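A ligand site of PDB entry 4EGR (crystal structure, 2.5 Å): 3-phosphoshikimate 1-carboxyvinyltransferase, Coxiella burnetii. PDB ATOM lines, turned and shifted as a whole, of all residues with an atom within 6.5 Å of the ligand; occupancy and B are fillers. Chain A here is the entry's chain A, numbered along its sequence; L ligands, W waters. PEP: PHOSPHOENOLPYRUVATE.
The side-chain carboxylate (OD2) of Asp 318 is in salt-bridge range of the guanidinium group (NH2) of Arg 197, 3.5 Å away. OG of Ser 97 is in hydrogen-bond range of N of Ala 100, at 3.1 Å. NE2 of His 28 lies within hydrogen-bond range of OG of Ser 97 (3.4 Å). N of Lys 24 is in hydrogen-bond range of OD1 of Asp 236, at 3.0 Å. The guanidinium group (NH1) of Arg 126 is in salt-bridge range of the side-chain carboxylate (OE1) of Glu 346, at 3.6 Å. OE2 of Glu 346 is in hydrogen-bond range of NE2 of His 389 (2.7 Å). ND1 of His 389 lies within hydrogen-bond range of OG of Ser 417, at 2.8 Å. The side-chain hydroxyl (OG1) of Thr 99 lies within hydrogen-bond range of the side-chain amide nitrogen (NE2) of Gln 172 (3.1 Å).
Water W1 lies within hydrogen-bond range of O1P of the ligand, NE2 of His 28, OG of Ser 97, NZ of Lys 24, OD2 of Asp 51 and OG1 of Thr 99.
The backbone NH (N) of Gly 98 is in hydrogen-bond range of an oxygen (O2P) of the ligand. An oxygen (O3P) of the ligand is in hydrogen-bond range of the side-chain amide nitrogen (NE2) of Gln 172, 3.4 Å away. The side-chain amino group (NZ) of Lys 24 lies within salt-bridge range of an oxygen (O2') of the ligand, 2.9 Å away. The backbone NH (N) of Thr 99 lies within hydrogen-bond range of an oxygen (O1P) of the ligand, at 3.4 Å. The guanidinium group (NH1) of Arg 126 lies within salt-bridge range of an oxygen (O2P) of the ligand. An oxygen (O2') of the ligand lies within salt-bridge range of the guanidinium group (NH2) of Arg 390 (2.5 Å). The side-chain hydroxyl of Thr 99 is in hydrogen-bond range of an oxygen (O1P) of the ligand (2.5 Å). NH1 of Arg 349 lies within salt-bridge range of O1 of the ligand (3.1 Å).
OD1 of Asp 318 lies close to O1 of the ligand. OE2 of Glu 346 sits close to O2 of the ligand, at 3.3 Å. O of Asn 96 touches O2P of the ligand (3.7 Å). Ser 97 touches the ligand (C to O2P, 3.9 Å). NE2 of His 389 touches O1 of the ligand, 3.7 Å away. Of the 25 residues printed, 12 come within 4 Å of the ligand. The nearest printed residue that does not touch the ligand is Asp 51 (4.2 Å).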
ATOM      1  N   LYS A  24      15.763  14.811 -30.370  1.00  0.00           N
ATOM      2  CA  LYS A  24      16.589  14.616 -29.191  1.00  0.00           C
ATOM      3  C   LYS A  24      16.485  13.187 -28.665  1.00  0.00           C
ATOM      4  O   LYS A  24      17.481  12.549 -28.406  1.00  0.00           O
ATOM      5  CB  LYS A  24      16.174  15.614 -28.103  1.00  0.00           C
ATOM      6  CG  LYS A  24      17.052  15.581 -26.874  1.00  0.00           C
ATOM      7  CD  LYS A  24      16.938  16.882 -26.079  1.00  0.00           C
ATOM      8  CE  LYS A  24      15.553  17.109 -25.477  1.00  0.00           C
ATOM      9  NZ  LYS A  24      15.171  16.034 -24.517  1.00  0.00           N
ATOM     10  N   SER A  25      15.265  12.727 -28.521  1.00  0.00           N
ATOM     11  CA  SER A  25      14.975  11.410 -28.032  1.00  0.00           C
ATOM     12  C   SER A  25      15.654  10.329 -28.854  1.00  0.00           C
ATOM     13  O   SER A  25      16.337   9.447 -28.303  1.00  0.00           O
ATOM     14  CB  SER A  25      13.471  11.165 -28.010  1.00  0.00           C
ATOM     15  OG  SER A  25      12.850  11.900 -26.983  1.00  0.00           O
ATOM     16  N   HIS A  28      19.588  10.410 -28.604  1.00  0.00           N
ATOM     17  CA  HIS A  28      20.238   9.841 -27.439  1.00  0.00           C
ATOM     18  C   HIS A  28      20.411   8.356 -27.559  1.00  0.00           C
ATOM     19  O   HIS A  28      21.473   7.775 -27.219  1.00  0.00           O
ATOM     20  CB  HIS A  28      19.424  10.097 -26.181  1.00  0.00           C
ATOM     21  CG  HIS A  28      19.594  11.479 -25.549  1.00  0.00           C
ATOM     22  ND1 HIS A  28      20.775  11.923 -25.085  1.00  0.00           N
ATOM     23  CD2 HIS A  28      18.647  12.419 -25.158  1.00  0.00           C
ATOM     24  CE1 HIS A  28      20.624  13.128 -24.506  1.00  0.00           C
ATOM     25  NE2 HIS A  28      19.320  13.432 -24.537  1.00  0.00           N
ATOM     26  N   ASP A  51      22.432  18.694 -24.642  1.00  0.00           N
ATOM     27  CA  ASP A  51      22.011  17.431 -24.048  1.00  0.00           C
ATOM     28  C   ASP A  51      22.591  16.253 -24.792  1.00  0.00           C
ATOM     29  O   ASP A  51      23.247  15.411 -24.165  1.00  0.00           O
ATOM     30  CB  ASP A  51      20.467  17.305 -23.944  1.00  0.00           C
ATOM     31  CG  ASP A  51      19.880  18.046 -22.718  1.00  0.00           C
ATOM     32  OD1 ASP A  51      20.637  18.772 -22.017  1.00  0.00           O
ATOM     33  OD2 ASP A  51      18.666  17.822 -22.428  1.00  0.00           O
ATOM     34  N   ASN A  96      22.590  18.864 -18.259  1.00  0.00           N
ATOM     35  CA  ASN A  96      21.208  19.155 -17.890  1.00  0.00           C
ATOM     36  C   ASN A  96      20.247  18.053 -18.294  1.00  0.00           C
ATOM     37  O   ASN A  96      19.034  18.209 -18.109  1.00  0.00           O
ATOM     38  CB  ASN A  96      20.798  20.452 -18.613  1.00  0.00           C
ATOM     39  CG  ASN A  96      19.467  20.995 -18.154  1.00  0.00           C
ATOM     40  OD1 ASN A  96      18.572  21.239 -18.973  1.00  0.00           O
ATOM     41  ND2 ASN A  96      19.321  21.196 -16.853  1.00  0.00           N
ATOM     42  N   SER A  97      20.788  16.934 -18.791  1.00  0.00           N
ATOM     43  CA  SER A  97      19.952  15.907 -19.413  1.00  0.00           C
ATOM     44  C   SER A  97      19.422  14.719 -18.586  1.00  0.00           C
ATOM     45  O   SER A  97      20.129  13.765 -18.309  1.00  0.00           O
ATOM     46  CB  SER A  97      20.655  15.367 -20.673  1.00  0.00           C
ATOM     47  OG  SER A  97      19.880  14.362 -21.292  1.00  0.00           O
ATOM     48  N   GLY A  98      18.120  14.764 -18.290  1.00  0.00           N
ATOM     49  CA  GLY A  98      17.467  13.687 -17.580  1.00  0.00           C
ATOM     50  C   GLY A  98      17.507  12.382 -18.376  1.00  0.00           C
ATOM     51  O   GLY A  98      17.799  11.327 -17.815  1.00  0.00           O
ATOM     52  N   THR A  99      17.242  12.441 -19.683  1.00  0.00           N
ATOM     53  CA  THR A  99      17.277  11.245 -20.540  1.00  0.00           C
ATOM     54  C   THR A  99      18.658  10.570 -20.473  1.00  0.00           C
ATOM     55  O   THR A  99      18.777   9.382 -20.269  1.00  0.00           O
ATOM     56  CB  THR A  99      16.972  11.602 -21.995  1.00  0.00           C
ATOM     57  OG1 THR A  99      15.800  12.414 -22.045  1.00  0.00           O
ATOM     58  CG2 THR A  99      16.774  10.333 -22.853  1.00  0.00           C
ATOM     59  N   ALA A 100      19.720  11.351 -20.584  1.00  0.00           N
ATOM     60  CA  ALA A 100      21.048  10.760 -20.528  1.00  0.00           C
ATOM     61  C   ALA A 100      21.254   9.992 -19.221  1.00  0.00           C
ATOM     62  O   ALA A 100      21.572   8.806 -19.233  1.00  0.00           O
ATOM     63  CB  ALA A 100      22.141  11.830 -20.685  1.00  0.00           C
ATOM     64  N   ARG A 102      19.257   8.776 -16.990  1.00  0.00           N
ATOM     65  CA  ARG A 102      18.409   7.628 -16.751  1.00  0.00           C
ATOM     66  C   ARG A 102      18.697   6.474 -17.731  1.00  0.00           C
ATOM     67  O   ARG A 102      18.633   5.301 -17.345  1.00  0.00           O
ATOM     68  CB  ARG A 102      16.927   8.047 -16.790  1.00  0.00           C
ATOM     69  CG  ARG A 102      16.529   9.114 -15.758  1.00  0.00           C
ATOM     70  CD  ARG A 102      15.008   9.127 -15.532  1.00  0.00           C
ATOM     71  NE  ARG A 102      14.496  10.030 -14.484  1.00  0.00           N
ATOM     72  CZ  ARG A 102      13.899  11.214 -14.678  1.00  0.00           C
ATOM     73  NH1 ARG A 102      13.739  11.712 -15.905  1.00  0.00           N
ATOM     74  NH2 ARG A 102      13.459  11.916 -13.651  1.00  0.00           N
ATOM     75  N   LEU A 123      19.706  18.917 -12.710  1.00  0.00           N
ATOM     76  CA  LEU A 123      19.663  17.494 -12.869  1.00  0.00           C
ATOM     77  C   LEU A 123      19.716  16.812 -11.489  1.00  0.00           C
ATOM     78  O   LEU A 123      19.113  15.748 -11.275  1.00  0.00           O
ATOM     79  CB  LEU A 123      20.835  17.036 -13.749  1.00  0.00           C
ATOM     80  CG  LEU A 123      20.703  15.607 -14.299  1.00  0.00           C
ATOM     81  CD1 LEU A 123      19.405  15.448 -15.085  1.00  0.00           C
ATOM     82  CD2 LEU A 123      21.898  15.266 -15.175  1.00  0.00           C
ATOM     83  N   ARG A 126      16.291  16.137  -9.957  1.00  0.00           N
ATOM     84  CA  ARG A 126      15.328  15.289 -10.643  1.00  0.00           C
ATOM     85  C   ARG A 126      15.266  13.887 -10.072  1.00  0.00           C
ATOM     86  O   ARG A 126      16.288  13.295  -9.744  1.00  0.00           O
ATOM     87  CB  ARG A 126      15.552  15.341 -12.163  1.00  0.00           C
ATOM     88  CG  ARG A 126      15.352  16.779 -12.627  1.00  0.00           C
ATOM     89  CD  ARG A 126      15.412  17.001 -14.113  1.00  0.00           C
ATOM     90  NE  ARG A 126      14.373  16.240 -14.759  1.00  0.00           N
ATOM     91  CZ  ARG A 126      14.287  16.102 -16.070  1.00  0.00           C
ATOM     92  NH1 ARG A 126      15.170  16.715 -16.844  1.00  0.00           N
ATOM     93  NH2 ARG A 126      13.328  15.355 -16.601  1.00  0.00           N
ATOM     94  N   GLN A 172      11.504   6.886 -20.591  1.00  0.00           N
ATOM     95  CA  GLN A 172      12.797   6.818 -19.982  1.00  0.00           C
ATOM     96  C   GLN A 172      12.928   5.576 -19.127  1.00  0.00           C
ATOM     97  O   GLN A 172      13.942   4.907 -19.161  1.00  0.00           O
ATOM     98  CB  GLN A 172      13.098   8.080 -19.186  1.00  0.00           C
ATOM     99  CG  GLN A 172      13.431   9.303 -20.043  1.00  0.00           C
ATOM    100  CD  GLN A 172      13.954  10.457 -19.202  1.00  0.00           C
ATOM    101  OE1 GLN A 172      14.439  10.244 -18.087  1.00  0.00           O
ATOM    102  NE2 GLN A 172      13.881  11.689 -19.734  1.00  0.00           N
ATOM    103  N   ARG A 197       6.457   7.033 -25.789  1.00  0.00           N
ATOM    104  CA  ARG A 197       7.230   7.019 -27.053  1.00  0.00           C
ATOM    105  C   ARG A 197       8.115   5.738 -27.220  1.00  0.00           C
ATOM    106  O   ARG A 197       8.799   5.282 -26.286  1.00  0.00           O
ATOM    107  CB  ARG A 197       8.024   8.304 -27.208  1.00  0.00           C
ATOM    108  CG  ARG A 197       8.947   8.599 -26.037  1.00  0.00           C
ATOM    109  CD  ARG A 197       9.577   9.971 -26.171  1.00  0.00           C
ATOM    110  NE  ARG A 197       8.624  11.033 -25.919  1.00  0.00           N
ATOM    111  CZ  ARG A 197       8.913  12.324 -25.906  1.00  0.00           C
ATOM    112  NH1 ARG A 197      10.164  12.756 -26.108  1.00  0.00           N
ATOM    113  NH2 ARG A 197       7.943  13.195 -25.665  1.00  0.00           N
ATOM    114  N   ASP A 236      12.851  16.910 -34.974  1.00  0.00           N
ATOM    115  CA  ASP A 236      12.180  16.777 -33.716  1.00  0.00           C
ATOM    116  C   ASP A 236      10.861  17.523 -33.817  1.00  0.00           C
ATOM    117  O   ASP A 236      10.835  18.721 -34.043  1.00  0.00           O
ATOM    118  CB  ASP A 236      13.021  17.373 -32.592  1.00  0.00           C
ATOM    119  CG  ASP A 236      12.645  16.839 -31.230  1.00  0.00           C
ATOM    120  OD1 ASP A 236      13.543  16.755 -30.361  1.00  0.00           O
ATOM    121  OD2 ASP A 236      11.459  16.494 -31.029  1.00  0.00           O
ATOM    122  N   SER A 238       8.995  18.105 -31.335  1.00  0.00           N
ATOM    123  CA  SER A 238       8.998  18.997 -30.166  1.00  0.00           C
ATOM    124  C   SER A 238       9.578  20.358 -30.556  1.00  0.00           C
ATOM    125  O   SER A 238       9.184  21.390 -29.992  1.00  0.00           O
ATOM    126  CB  SER A 238       9.760  18.398 -28.996  1.00  0.00           C
ATOM    127  OG  SER A 238       9.069  17.250 -28.539  1.00  0.00           O
ATOM    128  N   ILE A 317       3.558  15.733 -23.120  1.00  0.00           N
ATOM    129  CA  ILE A 317       4.158  16.294 -21.911  1.00  0.00           C
ATOM    130  C   ILE A 317       5.149  17.451 -22.186  1.00  0.00           C
ATOM    131  O   ILE A 317       5.064  18.501 -21.574  1.00  0.00           O
ATOM    132  CB  ILE A 317       4.787  15.152 -21.050  1.00  0.00           C
ATOM    133  CG1 ILE A 317       4.797  15.526 -19.597  1.00  0.00           C
ATOM    134  CG2 ILE A 317       6.158  14.716 -21.562  1.00  0.00           C
ATOM    135  CD1 ILE A 317       3.399  15.702 -19.025  1.00  0.00           C
ATOM    136  N   ASP A 318       6.046  17.259 -23.136  1.00  0.00           N
ATOM    137  CA  ASP A 318       7.020  18.283 -23.430  1.00  0.00           C
ATOM    138  C   ASP A 318       6.448  19.439 -24.235  1.00  0.00           C
ATOM    139  O   ASP A 318       7.080  20.466 -24.356  1.00  0.00           O
ATOM    140  CB  ASP A 318       8.195  17.679 -24.171  1.00  0.00           C
ATOM    141  CG  ASP A 318       8.940  16.655 -23.356  1.00  0.00           C
ATOM    142  OD1 ASP A 318       8.914  16.707 -22.090  1.00  0.00           O
ATOM    143  OD2 ASP A 318       9.588  15.797 -24.008  1.00  0.00           O
ATOM    144  N   LYS A 345      10.565  18.441 -14.052  1.00  0.00           N
ATOM    145  CA  LYS A 345      11.407  18.485 -15.258  1.00  0.00           C
ATOM    146  C   LYS A 345      12.608  19.426 -14.991  1.00  0.00           C
ATOM    147  O   LYS A 345      12.919  19.684 -13.841  1.00  0.00           O
ATOM    148  CB  LYS A 345      10.553  18.967 -16.440  1.00  0.00           C
ATOM    149  CG  LYS A 345       9.419  18.036 -16.826  1.00  0.00           C
ATOM    150  CD  LYS A 345       9.921  16.776 -17.548  1.00  0.00           C
ATOM    151  CE  LYS A 345       8.807  15.756 -17.834  1.00  0.00           C
ATOM    152  NZ  LYS A 345       9.167  14.622 -18.759  1.00  0.00           N
ATOM    153  N   GLU A 346      13.280  19.926 -16.047  1.00  0.00           N
ATOM    154  CA  GLU A 346      14.416  20.876 -15.903  1.00  0.00           C
ATOM    155  C   GLU A 346      14.075  21.845 -14.744  1.00  0.00           C
ATOM    156  O   GLU A 346      14.871  22.117 -13.836  1.00  0.00           O
ATOM    157  CB  GLU A 346      14.632  21.719 -17.191  1.00  0.00           C
ATOM    158  CG  GLU A 346      15.422  21.136 -18.368  1.00  0.00           C
ATOM    159  CD  GLU A 346      14.653  20.146 -19.264  1.00  0.00           C
ATOM    160  OE1 GLU A 346      13.752  19.391 -18.766  1.00  0.00           O
ATOM    161  OE2 GLU A 346      14.998  20.086 -20.490  1.00  0.00           O
ATOM    162  N   ARG A 349       7.691  23.208 -14.638  1.00  0.00           N
ATOM    163  CA  ARG A 349       7.092  23.874 -15.772  1.00  0.00           C
ATOM    164  C   ARG A 349       5.691  24.474 -15.560  1.00  0.00           C
ATOM    165  O   ARG A 349       5.310  25.385 -16.287  1.00  0.00           O
ATOM    166  CB  ARG A 349       7.128  22.953 -16.982  1.00  0.00           C
ATOM    167  CG  ARG A 349       8.559  22.768 -17.448  1.00  0.00           C
ATOM    168  CD  ARG A 349       8.729  21.765 -18.572  1.00  0.00           C
ATOM    169  NE  ARG A 349      10.081  21.853 -19.120  1.00  0.00           N
ATOM    170  CZ  ARG A 349      10.596  20.993 -20.003  1.00  0.00           C
ATOM    171  NH1 ARG A 349       9.914  19.958 -20.412  1.00  0.00           N
ATOM    172  NH2 ARG A 349      11.815  21.169 -20.455  1.00  0.00           N
ATOM    173  N   ASP A 388      15.072  27.022 -18.371  1.00  0.00           N
ATOM    174  CA  ASP A 388      14.450  25.923 -19.091  1.00  0.00           C
ATOM    175  C   ASP A 388      14.259  26.227 -20.564  1.00  0.00           C
ATOM    176  O   ASP A 388      13.591  27.170 -20.947  1.00  0.00           O
ATOM    177  CB  ASP A 388      13.138  25.520 -18.391  1.00  0.00           C
ATOM    178  CG  ASP A 388      12.484  24.320 -19.016  1.00  0.00           C
ATOM    179  OD1 ASP A 388      12.613  24.112 -20.256  1.00  0.00           O
ATOM    180  OD2 ASP A 388      11.802  23.603 -18.265  1.00  0.00           O
ATOM    181  N   HIS A 389      14.819  25.377 -21.397  1.00  0.00           N
ATOM    182  CA  HIS A 389      14.782  25.618 -22.825  1.00  0.00           C
ATOM    183  C   HIS A 389      13.402  25.708 -23.406  1.00  0.00           C
ATOM    184  O   HIS A 389      13.152  26.520 -24.307  1.00  0.00           O
ATOM    185  CB  HIS A 389      15.648  24.601 -23.564  1.00  0.00           C
ATOM    186  CG  HIS A 389      15.143  23.202 -23.478  1.00  0.00           C
ATOM    187  ND1 HIS A 389      14.827  22.501 -24.579  1.00  0.00           N
ATOM    188  CD2 HIS A 389      14.918  22.359 -22.375  1.00  0.00           C
ATOM    189  CE1 HIS A 389      14.370  21.261 -24.206  1.00  0.00           C
ATOM    190  NE2 HIS A 389      14.420  21.172 -22.859  1.00  0.00           N
ATOM    191  N   ARG A 390      12.472  24.895 -22.936  1.00  0.00           N
ATOM    192  CA  ARG A 390      11.104  24.979 -23.479  1.00  0.00           C
ATOM    193  C   ARG A 390      10.331  26.227 -22.974  1.00  0.00           C
ATOM    194  O   ARG A 390       9.534  26.819 -23.709  1.00  0.00           O
ATOM    195  CB  ARG A 390      10.317  23.688 -23.263  1.00  0.00           C
ATOM    196  CG  ARG A 390      10.996  22.490 -23.910  1.00  0.00           C
ATOM    197  CD  ARG A 390      10.088  21.264 -24.129  1.00  0.00           C
ATOM    198  NE  ARG A 390      10.927  20.143 -24.521  1.00  0.00           N
ATOM    199  CZ  ARG A 390      11.430  19.971 -25.747  1.00  0.00           C
ATOM    200  NH1 ARG A 390      11.100  20.773 -26.750  1.00  0.00           N
ATOM    201  NH2 ARG A 390      12.261  18.951 -25.977  1.00  0.00           N
ATOM    202  N   SER A 417      18.369  21.810 -26.657  1.00  0.00           N
ATOM    203  CA  SER A 417      17.597  21.064 -27.684  1.00  0.00           C
ATOM    204  C   SER A 417      17.419  21.772 -29.017  1.00  0.00           C
ATOM    205  O   SER A 417      16.916  21.163 -29.973  1.00  0.00           O
ATOM    206  CB  SER A 417      16.166  20.727 -27.191  1.00  0.00           C
ATOM    207  OG  SER A 417      15.282  21.872 -27.264  1.00  0.00           O
HETATM  208  C1  PEP L   1      12.518  17.578 -22.766  1.00  0.00           C
HETATM  209  O1  PEP L   1      11.859  18.521 -22.273  1.00  0.00           O
HETATM  210  O2' PEP L   1      12.717  17.489 -24.003  1.00  0.00           O
HETATM  211  C2  PEP L   1      13.077  16.566 -21.879  1.00  0.00           C
HETATM  212  C3  PEP L   1      12.545  15.364 -21.837  1.00  0.00           C
HETATM  213  O2  PEP L   1      14.227  16.889 -21.042  1.00  0.00           O
HETATM  214  P   PEP L   1      15.022  15.712 -20.284  1.00  0.00           P
HETATM  215  O1P PEP L   1      15.556  14.861 -21.406  1.00  0.00           O
HETATM  216  O2P PEP L   1      16.080  16.441 -19.488  1.00  0.00           O
HETATM  217  O3P PEP L   1      13.957  15.037 -19.446  1.00  0.00           O
HETATM  218  O   HOH W   1      17.539  15.076 -22.983  1.00  0.00           O
HETATM  219  O   HOH W   2      17.419  18.656 -20.136  1.00  0.00           O
